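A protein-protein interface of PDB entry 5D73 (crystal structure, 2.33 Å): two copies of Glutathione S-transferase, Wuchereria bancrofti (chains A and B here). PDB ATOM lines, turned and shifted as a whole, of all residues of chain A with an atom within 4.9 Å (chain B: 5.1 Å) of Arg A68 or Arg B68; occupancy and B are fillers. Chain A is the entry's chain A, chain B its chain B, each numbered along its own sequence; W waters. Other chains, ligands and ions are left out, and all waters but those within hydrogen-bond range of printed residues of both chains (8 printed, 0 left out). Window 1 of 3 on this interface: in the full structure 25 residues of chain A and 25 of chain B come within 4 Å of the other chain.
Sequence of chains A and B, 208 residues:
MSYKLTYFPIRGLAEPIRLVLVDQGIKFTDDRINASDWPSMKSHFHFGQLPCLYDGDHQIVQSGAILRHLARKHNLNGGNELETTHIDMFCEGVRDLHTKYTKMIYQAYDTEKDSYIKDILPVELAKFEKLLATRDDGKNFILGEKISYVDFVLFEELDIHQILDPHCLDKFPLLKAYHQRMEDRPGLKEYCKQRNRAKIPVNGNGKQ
The guanidinium group (NE) of Arg A68 sits close to the backbone carbonyl oxygen (O) of Gly A64 (3.4 Å).
The guanidinium group of Arg A72 is in hydrogen-bond range of the backbone carbonyl oxygen of Arg A68 (3.3 Å).
NH1 of Arg A68 lies within salt-bridge range of OD1 of Asp A88.
The backbone carbonyl oxygen (O) of Gly B64 lies close to the guanidinium group (NH2) of Arg B68, at 3.2 Å.
O of Arg B68 is in hydrogen-bond range of NH1 of Arg B72 (3.4 Å).
NH1 of Arg B68 lies within salt-bridge range of OD1 of Asp B88 (3.9 Å).
Of chain A, only Arg A68, Asp A88 and Glu A92 come within 4 Å of Arg B68.
Of the printed residues of chain A, Glu B92 touches Arg A68 (3.8 Å) and Arg A95 (3.5 Å).
Of the printed residues of chain B, Glu A92 touches Arg B68 (3.9 Å).
Of the printed residues of chain A, Ala B65 touches Asp A88 (3.6 Å).
Leu B70 touches none of the printed residues of chain A.
Of the 13 printed residues of chain B, 4 touch a printed residue of chain A.
Printed residues of chain B that touch a printed residue of chain A: Ala B65, Arg B68, Asp B88 and Glu B92.
Hydrophobic or aromatic side chains of chain B within 4 Å of the printed part of chain A: Ala B65.
Printed residues of chain A that touch a printed residue of chain B: Ala A65, Arg A68, Asp A88, Glu A92 and Arg A95.
Along chain A the printed residues that touch a printed residue of chain B span positions 65 to 95.
Among the printed residues, 8 pairs touch across the chains.
The side-chain carboxylate (OD2) of Asp B88 lies within salt-bridge range of the guanidinium group (NE) of Arg A68, 2.6 Å away.
The guanidinium group (NH2) of Arg A68 is in salt-bridge range of the side-chain carboxylate (OE2) of Glu B92, 3.9 Å away.
NE of Arg B68 is in salt-bridge range of OD2 of Asp A88 (2.7 Å).
OE2 of Glu B92 is in salt-bridge range of NH1 of Arg A95 (3.5 Å).
Ala A65 touches Asp B88, and with the chains exchanged Asp A88 touches Ala B65.
Arg A68 touches its own counterpart, Arg B68.
Arg A68 touches Asp B88, and with the chains exchanged Asp A88 touches Arg B68.
Arg A68 touches Glu B92, and with the chains exchanged Glu A92 touches Arg B68.
Of the 8 pairs that touch across the chains among the printed residues, 7 have their exchanged pair printed and touching as well.
Asp B88 touches Ala A65.
NH1 of Arg B68 touches NH2 of Arg A68, at 3.5 Å.
Ala B65 touches Asp A88 (CA to OD2, 3.6 Å).
Glu A92 touches Arg B68.
Water W4 lies within hydrogen-bond range of NH1 of Arg A95 (2.6 Å), OE2 of Glu A92 (2.7 Å), OE2 of Glu B92 (2.8 Å) and NH1 of Arg A68 (3.1 Å).
Water W1 lies within hydrogen-bond range of O of Ala B65, NH2 of Arg B72 and OD2 of Asp A88.
Water W8 lies within hydrogen-bond range of the side-chain carboxylate of Asp A88 (2.7 Å) and the guanidinium group of Arg B72 (3.0 Å).
Water W5 lies within hydrogen-bond range of the side-chain carboxylate of Glu B92, the backbone NH of Gly A64 and the guanidinium group of Arg A95.
Water W7 lies within hydrogen-bond range of OD2 of Asp B88 (2.7 Å) and NH1 of Arg A72 (3.0 Å).
Water W6 lies within hydrogen-bond range of the side-chain carboxylate (OE1) of Glu B92 (2.9 Å), the guanidinium group (NH1) of Arg B68 (3.0 Å) and the side-chain carboxylate (OE1) of Glu A92 (3.1 Å).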
ATOM      1  N   GLY A  64       7.600 -13.364   2.058  1.00  0.00           N
ATOM      2  CA  GLY A  64       7.236 -12.178   2.820  1.00  0.00           C
ATOM      3  C   GLY A  64       8.404 -11.484   3.487  1.00  0.00           C
ATOM      4  O   GLY A  64       8.485 -10.236   3.487  1.00  0.00           O
ATOM      5  N   ALA A  65       9.316 -12.282   4.062  1.00  0.00           N
ATOM      6  CA  ALA A  65      10.510 -11.730   4.714  1.00  0.00           C
ATOM      7  C   ALA A  65      11.449 -11.040   3.701  1.00  0.00           C
ATOM      8  O   ALA A  65      12.076 -10.016   4.021  1.00  0.00           O
ATOM      9  CB  ALA A  65      11.261 -12.808   5.535  1.00  0.00           C
ATOM     10  N   ILE A  66      11.518 -11.622   2.500  1.00  0.00           N
ATOM     11  CA  ILE A  66      12.306 -11.098   1.399  1.00  0.00           C
ATOM     12  C   ILE A  66      11.735  -9.747   0.980  1.00  0.00           C
ATOM     13  O   ILE A  66      12.457  -8.769   0.849  1.00  0.00           O
ATOM     14  CB  ILE A  66      12.312 -12.070   0.192  1.00  0.00           C
ATOM     15  CG1 ILE A  66      13.047 -13.383   0.532  1.00  0.00           C
ATOM     16  CG2 ILE A  66      12.983 -11.445  -1.016  1.00  0.00           C
ATOM     17  CD1 ILE A  66      12.719 -14.582  -0.347  1.00  0.00           C
ATOM     18  N   LEU A  67      10.431  -9.702   0.773  1.00  0.00           N
ATOM     19  CA  LEU A  67       9.768  -8.451   0.324  1.00  0.00           C
ATOM     20  C   LEU A  67       9.938  -7.339   1.352  1.00  0.00           C
ATOM     21  O   LEU A  67      10.340  -6.217   0.995  1.00  0.00           O
ATOM     22  CB  LEU A  67       8.293  -8.691   0.000  1.00  0.00           C
ATOM     23  CG  LEU A  67       8.054  -9.419  -1.331  1.00  0.00           C
ATOM     24  CD1 LEU A  67       6.678 -10.097  -1.380  1.00  0.00           C
ATOM     25  CD2 LEU A  67       8.152  -8.451  -2.490  1.00  0.00           C
ATOM     26  N   ARG A  68       9.662  -7.658   2.618  1.00  0.00           N
ATOM     27  CA  ARG A  68       9.787  -6.653   3.681  1.00  0.00           C
ATOM     28  C   ARG A  68      11.249  -6.146   3.936  1.00  0.00           C
ATOM     29  O   ARG A  68      11.476  -4.948   4.262  1.00  0.00           O
ATOM     30  CB  ARG A  68       9.148  -7.172   4.956  1.00  0.00           C
ATOM     31  CG  ARG A  68       7.623  -7.158   4.914  1.00  0.00           C
ATOM     32  CD  ARG A  68       6.990  -7.652   6.202  1.00  0.00           C
ATOM     33  NE  ARG A  68       7.159  -9.109   6.411  1.00  0.00           N
ATOM     34  CZ  ARG A  68       6.347 -10.065   5.956  1.00  0.00           C
ATOM     35  NH1 ARG A  68       5.262  -9.775   5.203  1.00  0.00           N
ATOM     36  NH2 ARG A  68       6.635 -11.330   6.235  1.00  0.00           N
ATOM     37  N   HIS A  69      12.221  -7.052   3.769  1.00  0.00           N
ATOM     38  CA  HIS A  69      13.660  -6.706   3.810  1.00  0.00           C
ATOM     39  C   HIS A  69      14.029  -5.731   2.703  1.00  0.00           C
ATOM     40  O   HIS A  69      14.720  -4.700   2.939  1.00  0.00           O
ATOM     41  CB  HIS A  69      14.512  -7.988   3.698  1.00  0.00           C
ATOM     42  CG  HIS A  69      15.967  -7.759   3.455  1.00  0.00           C
ATOM     43  ND1 HIS A  69      16.817  -7.258   4.413  1.00  0.00           N
ATOM     44  CD2 HIS A  69      16.748  -8.049   2.383  1.00  0.00           C
ATOM     45  CE1 HIS A  69      18.049  -7.223   3.943  1.00  0.00           C
ATOM     46  NE2 HIS A  69      18.033  -7.679   2.707  1.00  0.00           N
ATOM     47  N   LEU A  70      13.576  -6.062   1.500  1.00  0.00           N
ATOM     48  CA  LEU A  70      13.821  -5.212   0.349  1.00  0.00           C
ATOM     49  C   LEU A  70      13.169  -3.854   0.511  1.00  0.00           C
ATOM     50  O   LEU A  70      13.793  -2.835   0.214  1.00  0.00           O
ATOM     51  CB  LEU A  70      13.353  -5.867  -0.948  1.00  0.00           C
ATOM     52  CG  LEU A  70      14.180  -7.058  -1.398  1.00  0.00           C
ATOM     53  CD1 LEU A  70      13.563  -7.627  -2.663  1.00  0.00           C
ATOM     54  CD2 LEU A  70      15.622  -6.675  -1.652  1.00  0.00           C
ATOM     55  N   ALA A  71      11.930  -3.854   1.002  1.00  0.00           N
ATOM     56  CA  ALA A  71      11.223  -2.605   1.359  1.00  0.00           C
ATOM     57  C   ALA A  71      12.063  -1.667   2.244  1.00  0.00           C
ATOM     58  O   ALA A  71      12.154  -0.468   1.971  1.00  0.00           O
ATOM     59  CB  ALA A  71       9.897  -2.916   2.039  1.00  0.00           C
ATOM     60  N   ARG A  72      12.647  -2.240   3.300  1.00  0.00           N
ATOM     61  CA  ARG A  72      13.533  -1.501   4.202  1.00  0.00           C
ATOM     62  C   ARG A  72      14.883  -1.084   3.553  1.00  0.00           C
ATOM     63  O   ARG A  72      15.408  -0.041   3.912  1.00  0.00           O
ATOM     64  CB  ARG A  72      13.839  -2.317   5.468  1.00  0.00           C
ATOM     65  CG  ARG A  72      12.677  -2.549   6.438  1.00  0.00           C
ATOM     66  CD  ARG A  72      13.165  -3.192   7.739  1.00  0.00           C
ATOM     67  NE  ARG A  72      13.648  -4.581   7.568  1.00  0.00           N
ATOM     68  CZ  ARG A  72      12.883  -5.671   7.470  1.00  0.00           C
ATOM     69  NH1 ARG A  72      11.540  -5.591   7.512  1.00  0.00           N
ATOM     70  NH2 ARG A  72      13.453  -6.867   7.332  1.00  0.00           N
ATOM     71  N   ASP A  88       1.530  -3.405   4.841  1.00  0.00           N
ATOM     72  CA  ASP A  88       1.616  -4.799   5.304  1.00  0.00           C
ATOM     73  C   ASP A  88       0.223  -5.483   5.380  1.00  0.00           C
ATOM     74  O   ASP A  88       0.027  -6.616   4.957  1.00  0.00           O
ATOM     75  CB  ASP A  88       2.310  -4.843   6.663  1.00  0.00           C
ATOM     76  CG  ASP A  88       2.775  -6.227   7.056  1.00  0.00           C
ATOM     77  OD1 ASP A  88       2.568  -7.279   6.381  1.00  0.00           O
ATOM     78  OD2 ASP A  88       3.395  -6.259   8.111  1.00  0.00           O
ATOM     79  N   GLU A  92      -0.794  -8.627   3.104  1.00  0.00           N
ATOM     80  CA  GLU A  92      -1.375  -9.832   3.665  1.00  0.00           C
ATOM     81  C   GLU A  92      -2.749 -10.243   3.065  1.00  0.00           C
ATOM     82  O   GLU A  92      -3.040 -11.418   2.918  1.00  0.00           O
ATOM     83  CB  GLU A  92      -1.446  -9.717   5.177  1.00  0.00           C
ATOM     84  CG  GLU A  92      -0.101  -9.819   5.860  1.00  0.00           C
ATOM     85  CD  GLU A  92       0.500 -11.209   5.731  1.00  0.00           C
ATOM     86  OE1 GLU A  92       0.127 -12.120   6.470  1.00  0.00           O
ATOM     87  OE2 GLU A  92       1.325 -11.401   4.838  1.00  0.00           O
ATOM     88  N   ARG A  95      -2.116 -11.798  -0.238  1.00  0.00           N
ATOM     89  CA  ARG A  95      -1.618 -13.151  -0.078  1.00  0.00           C
ATOM     90  C   ARG A  95      -2.722 -14.139   0.279  1.00  0.00           C
ATOM     91  O   ARG A  95      -2.650 -15.293  -0.075  1.00  0.00           O
ATOM     92  CB  ARG A  95      -0.533 -13.152   0.982  1.00  0.00           C
ATOM     93  CG  ARG A  95       0.676 -12.283   0.611  1.00  0.00           C
ATOM     94  CD  ARG A  95       1.835 -12.468   1.582  1.00  0.00           C
ATOM     95  NE  ARG A  95       2.256 -13.881   1.587  1.00  0.00           N
ATOM     96  CZ  ARG A  95       3.428 -14.359   1.998  1.00  0.00           C
ATOM     97  NH1 ARG A  95       4.373 -13.562   2.460  1.00  0.00           N
ATOM     98  NH2 ARG A  95       3.659 -15.666   1.931  1.00  0.00           N
ATOM     99  N   TYR A 149       6.499  -1.407  -1.750  1.00  0.00           N
ATOM    100  CA  TYR A 149       6.634  -2.798  -2.201  1.00  0.00           C
ATOM    101  C   TYR A 149       5.293  -3.444  -2.505  1.00  0.00           C
ATOM    102  O   TYR A 149       5.197  -4.210  -3.469  1.00  0.00           O
ATOM    103  CB  TYR A 149       7.447  -3.676  -1.227  1.00  0.00           C
ATOM    104  CG  TYR A 149       6.739  -4.068   0.083  1.00  0.00           C
ATOM    105  CD1 TYR A 149       6.696  -3.195   1.160  1.00  0.00           C
ATOM    106  CD2 TYR A 149       6.147  -5.337   0.244  1.00  0.00           C
ATOM    107  CE1 TYR A 149       6.052  -3.534   2.345  1.00  0.00           C
ATOM    108  CE2 TYR A 149       5.493  -5.688   1.438  1.00  0.00           C
ATOM    109  CZ  TYR A 149       5.454  -4.771   2.477  1.00  0.00           C
ATOM    110  OH  TYR A 149       4.884  -5.094   3.699  1.00  0.00           O
ATOM    111  N   GLY B  64      -0.424 -11.011  11.222  1.00  0.00           N
ATOM    112  CA  GLY B  64       0.939 -10.643  10.893  1.00  0.00           C
ATOM    113  C   GLY B  64       1.239  -9.169  10.851  1.00  0.00           C
ATOM    114  O   GLY B  64       2.272  -8.749  11.328  1.00  0.00           O
ATOM    115  N   ALA B  65       0.352  -8.368  10.284  1.00  0.00           N
ATOM    116  CA  ALA B  65       0.554  -6.931  10.241  1.00  0.00           C
ATOM    117  C   ALA B  65       0.441  -6.362  11.662  1.00  0.00           C
ATOM    118  O   ALA B  65       1.223  -5.481  12.049  1.00  0.00           O
ATOM    119  CB  ALA B  65      -0.442  -6.281   9.291  1.00  0.00           C
ATOM    120  N   ILE B  66      -0.490  -6.929  12.458  1.00  0.00           N
ATOM    121  CA  ILE B  66      -0.659  -6.543  13.876  1.00  0.00           C
ATOM    122  C   ILE B  66       0.586  -6.821  14.686  1.00  0.00           C
ATOM    123  O   ILE B  66       1.004  -5.985  15.516  1.00  0.00           O
ATOM    124  CB  ILE B  66      -1.840  -7.263  14.562  1.00  0.00           C
ATOM    125  CG1 ILE B  66      -3.157  -6.835  13.928  1.00  0.00           C
ATOM    126  CG2 ILE B  66      -1.886  -6.917  16.057  1.00  0.00           C
ATOM    127  CD1 ILE B  66      -4.348  -7.651  14.386  1.00  0.00           C
ATOM    128  N   LEU B  67       1.158  -7.996  14.472  1.00  0.00           N
ATOM    129  CA  LEU B  67       2.331  -8.404  15.244  1.00  0.00           C
ATOM    130  C   LEU B  67       3.521  -7.501  14.981  1.00  0.00           C
ATOM    131  O   LEU B  67       4.139  -7.003  15.907  1.00  0.00           O
ATOM    132  CB  LEU B  67       2.689  -9.867  14.981  1.00  0.00           C
ATOM    133  CG  LEU B  67       1.814 -10.887  15.705  1.00  0.00           C
ATOM    134  CD1 LEU B  67       1.947 -12.278  15.075  1.00  0.00           C
ATOM    135  CD2 LEU B  67       2.166 -10.970  17.180  1.00  0.00           C
ATOM    136  N   ARG B  68       3.826  -7.289  13.715  1.00  0.00           N
ATOM    137  CA  ARG B  68       4.986  -6.500  13.329  1.00  0.00           C
ATOM    138  C   ARG B  68       4.794  -5.029  13.691  1.00  0.00           C
ATOM    139  O   ARG B  68       5.750  -4.331  13.974  1.00  0.00           O
ATOM    140  CB  ARG B  68       5.284  -6.693  11.816  1.00  0.00           C
ATOM    141  CG  ARG B  68       5.776  -8.089  11.438  1.00  0.00           C
ATOM    142  CD  ARG B  68       6.026  -8.252   9.930  1.00  0.00           C
ATOM    143  NE  ARG B  68       4.763  -8.329   9.198  1.00  0.00           N
ATOM    144  CZ  ARG B  68       4.136  -9.440   8.840  1.00  0.00           C
ATOM    145  NH1 ARG B  68       4.664 -10.643   9.054  1.00  0.00           N
ATOM    146  NH2 ARG B  68       2.957  -9.369   8.233  1.00  0.00           N
ATOM    147  N   HIS B  69       3.556  -4.552  13.658  1.00  0.00           N
ATOM    148  CA  HIS B  69       3.227  -3.218  14.178  1.00  0.00           C
ATOM    149  C   HIS B  69       3.615  -3.101  15.688  1.00  0.00           C
ATOM    150  O   HIS B  69       4.332  -2.195  16.093  1.00  0.00           O
ATOM    151  CB  HIS B  69       1.734  -2.890  13.997  1.00  0.00           C
ATOM    152  CG  HIS B  69       1.302  -1.652  14.736  1.00  0.00           C
ATOM    153  ND1 HIS B  69       1.757  -0.397  14.418  1.00  0.00           N
ATOM    154  CD2 HIS B  69       0.460  -1.484  15.782  1.00  0.00           C
ATOM    155  CE1 HIS B  69       1.212   0.496  15.224  1.00  0.00           C
ATOM    156  NE2 HIS B  69       0.405  -0.137  16.055  1.00  0.00           N
ATOM    157  N   LEU B  70       3.122  -4.036  16.492  1.00  0.00           N
ATOM    158  CA  LEU B  70       3.474  -4.100  17.916  1.00  0.00           C
ATOM    159  C   LEU B  70       4.989  -4.215  18.137  1.00  0.00           C
ATOM    160  O   LEU B  70       5.533  -3.622  19.078  1.00  0.00           O
ATOM    161  CB  LEU B  70       2.745  -5.243  18.606  1.00  0.00           C
ATOM    162  CG  LEU B  70       1.264  -5.006  18.889  1.00  0.00           C
ATOM    163  CD1 LEU B  70       0.584  -6.252  19.480  1.00  0.00           C
ATOM    164  CD2 LEU B  70       1.059  -3.810  19.807  1.00  0.00           C
ATOM    165  N   ALA B  71       5.663  -4.947  17.252  1.00  0.00           N
ATOM    166  CA  ALA B  71       7.106  -5.149  17.359  1.00  0.00           C
ATOM    167  C   ALA B  71       7.860  -3.839  17.251  1.00  0.00           C
ATOM    168  O   ALA B  71       8.750  -3.557  18.056  1.00  0.00           O
ATOM    169  CB  ALA B  71       7.575  -6.091  16.279  1.00  0.00           C
ATOM    170  N   ARG B  72       7.511  -3.044  16.237  1.00  0.00           N
ATOM    171  CA  ARG B  72       8.176  -1.755  16.020  1.00  0.00           C
ATOM    172  C   ARG B  72       7.847  -0.785  17.138  1.00  0.00           C
ATOM    173  O   ARG B  72       8.728  -0.144  17.668  1.00  0.00           O
ATOM    174  CB  ARG B  72       7.804  -1.155  14.663  1.00  0.00           C
ATOM    175  CG  ARG B  72       8.381  -1.928  13.481  1.00  0.00           C
ATOM    176  CD  ARG B  72       8.055  -1.253  12.175  1.00  0.00           C
ATOM    177  NE  ARG B  72       6.611  -1.154  11.960  1.00  0.00           N
ATOM    178  CZ  ARG B  72       5.835  -2.040  11.333  1.00  0.00           C
ATOM    179  NH1 ARG B  72       6.320  -3.155  10.803  1.00  0.00           N
ATOM    180  NH2 ARG B  72       4.542  -1.777  11.185  1.00  0.00           N
ATOM    181  N   ASN B  77      11.470  -5.972  17.916  1.00  0.00           N
ATOM    182  CA  ASN B  77      11.721  -6.321  16.492  1.00  0.00           C
ATOM    183  C   ASN B  77      13.179  -6.496  16.105  1.00  0.00           C
ATOM    184  O   ASN B  77      13.519  -6.401  14.930  1.00  0.00           O
ATOM    185  CB  ASN B  77      11.082  -5.237  15.595  1.00  0.00           C
ATOM    186  CG  ASN B  77      10.697  -5.741  14.217  1.00  0.00           C
ATOM    187  OD1 ASN B  77      10.443  -6.914  14.002  1.00  0.00           O
ATOM    188  ND2 ASN B  77      10.669  -4.831  13.267  1.00  0.00           N
ATOM    189  N   ASP B  88      11.505 -12.323  11.213  1.00  0.00           N
ATOM    190  CA  ASP B  88      10.424 -12.349  10.233  1.00  0.00           C
ATOM    191  C   ASP B  88      10.421 -13.692   9.495  1.00  0.00           C
ATOM    192  O   ASP B  88       9.392 -14.331   9.368  1.00  0.00           O
ATOM    193  CB  ASP B  88      10.583 -11.204   9.226  1.00  0.00           C
ATOM    194  CG  ASP B  88       9.339 -10.941   8.399  1.00  0.00           C
ATOM    195  OD1 ASP B  88       8.348 -11.678   8.455  1.00  0.00           O
ATOM    196  OD2 ASP B  88       9.346  -9.950   7.641  1.00  0.00           O
ATOM    197  N   GLU B  92       7.424 -16.530   9.778  1.00  0.00           N
ATOM    198  CA  GLU B  92       6.777 -17.081   8.593  1.00  0.00           C
ATOM    199  C   GLU B  92       6.904 -18.604   8.509  1.00  0.00           C
ATOM    200  O   GLU B  92       6.030 -19.270   7.973  1.00  0.00           O
ATOM    201  CB  GLU B  92       7.325 -16.438   7.329  1.00  0.00           C
ATOM    202  CG  GLU B  92       6.869 -15.016   7.088  1.00  0.00           C
ATOM    203  CD  GLU B  92       5.369 -14.895   6.801  1.00  0.00           C
ATOM    204  OE1 GLU B  92       4.587 -14.862   7.747  1.00  0.00           O
ATOM    205  OE2 GLU B  92       4.914 -14.797   5.649  1.00  0.00           O
ATOM    206  N   TYR B 149       9.053 -10.348  19.243  1.00  0.00           N
ATOM    207  CA  TYR B 149       7.649 -10.798  19.007  1.00  0.00           C
ATOM    208  C   TYR B 149       7.516 -12.286  18.591  1.00  0.00           C
ATOM    209  O   TYR B 149       6.474 -12.954  18.872  1.00  0.00           O
ATOM    210  CB  TYR B 149       6.885  -9.868  18.004  1.00  0.00           C
ATOM    211  CG  TYR B 149       7.248 -10.019  16.523  1.00  0.00           C
ATOM    212  CD1 TYR B 149       8.411  -9.443  16.016  1.00  0.00           C
ATOM    213  CD2 TYR B 149       6.432 -10.719  15.635  1.00  0.00           C
ATOM    214  CE1 TYR B 149       8.775  -9.590  14.691  1.00  0.00           C
ATOM    215  CE2 TYR B 149       6.780 -10.868  14.296  1.00  0.00           C
ATOM    216  CZ  TYR B 149       7.950 -10.293  13.818  1.00  0.00           C
ATOM    217  OH  TYR B 149       8.336 -10.374  12.479  1.00  0.00           O
HETATM  218  O   HOH W   1       2.483  -4.015  10.222  1.00  0.00           O
HETATM  219  O   HOH W   2      -1.588 -11.763   8.407  1.00  0.00           O
HETATM  220  O   HOH W   3      12.154  -9.131   6.752  1.00  0.00           O
HETATM  221  O   HOH W   4       3.784 -12.424   4.679  1.00  0.00           O
HETATM  222  O   HOH W   5       6.351 -15.620   3.541  1.00  0.00           O
HETATM  223  O   HOH W   6       2.709 -12.741   8.108  1.00  0.00           O
HETATM  224  O   HOH W   7       9.845  -7.609   8.930  1.00  0.00           O
HETATM  225  O   HOH W   8       5.480  -4.613   8.315  1.00  0.00           O
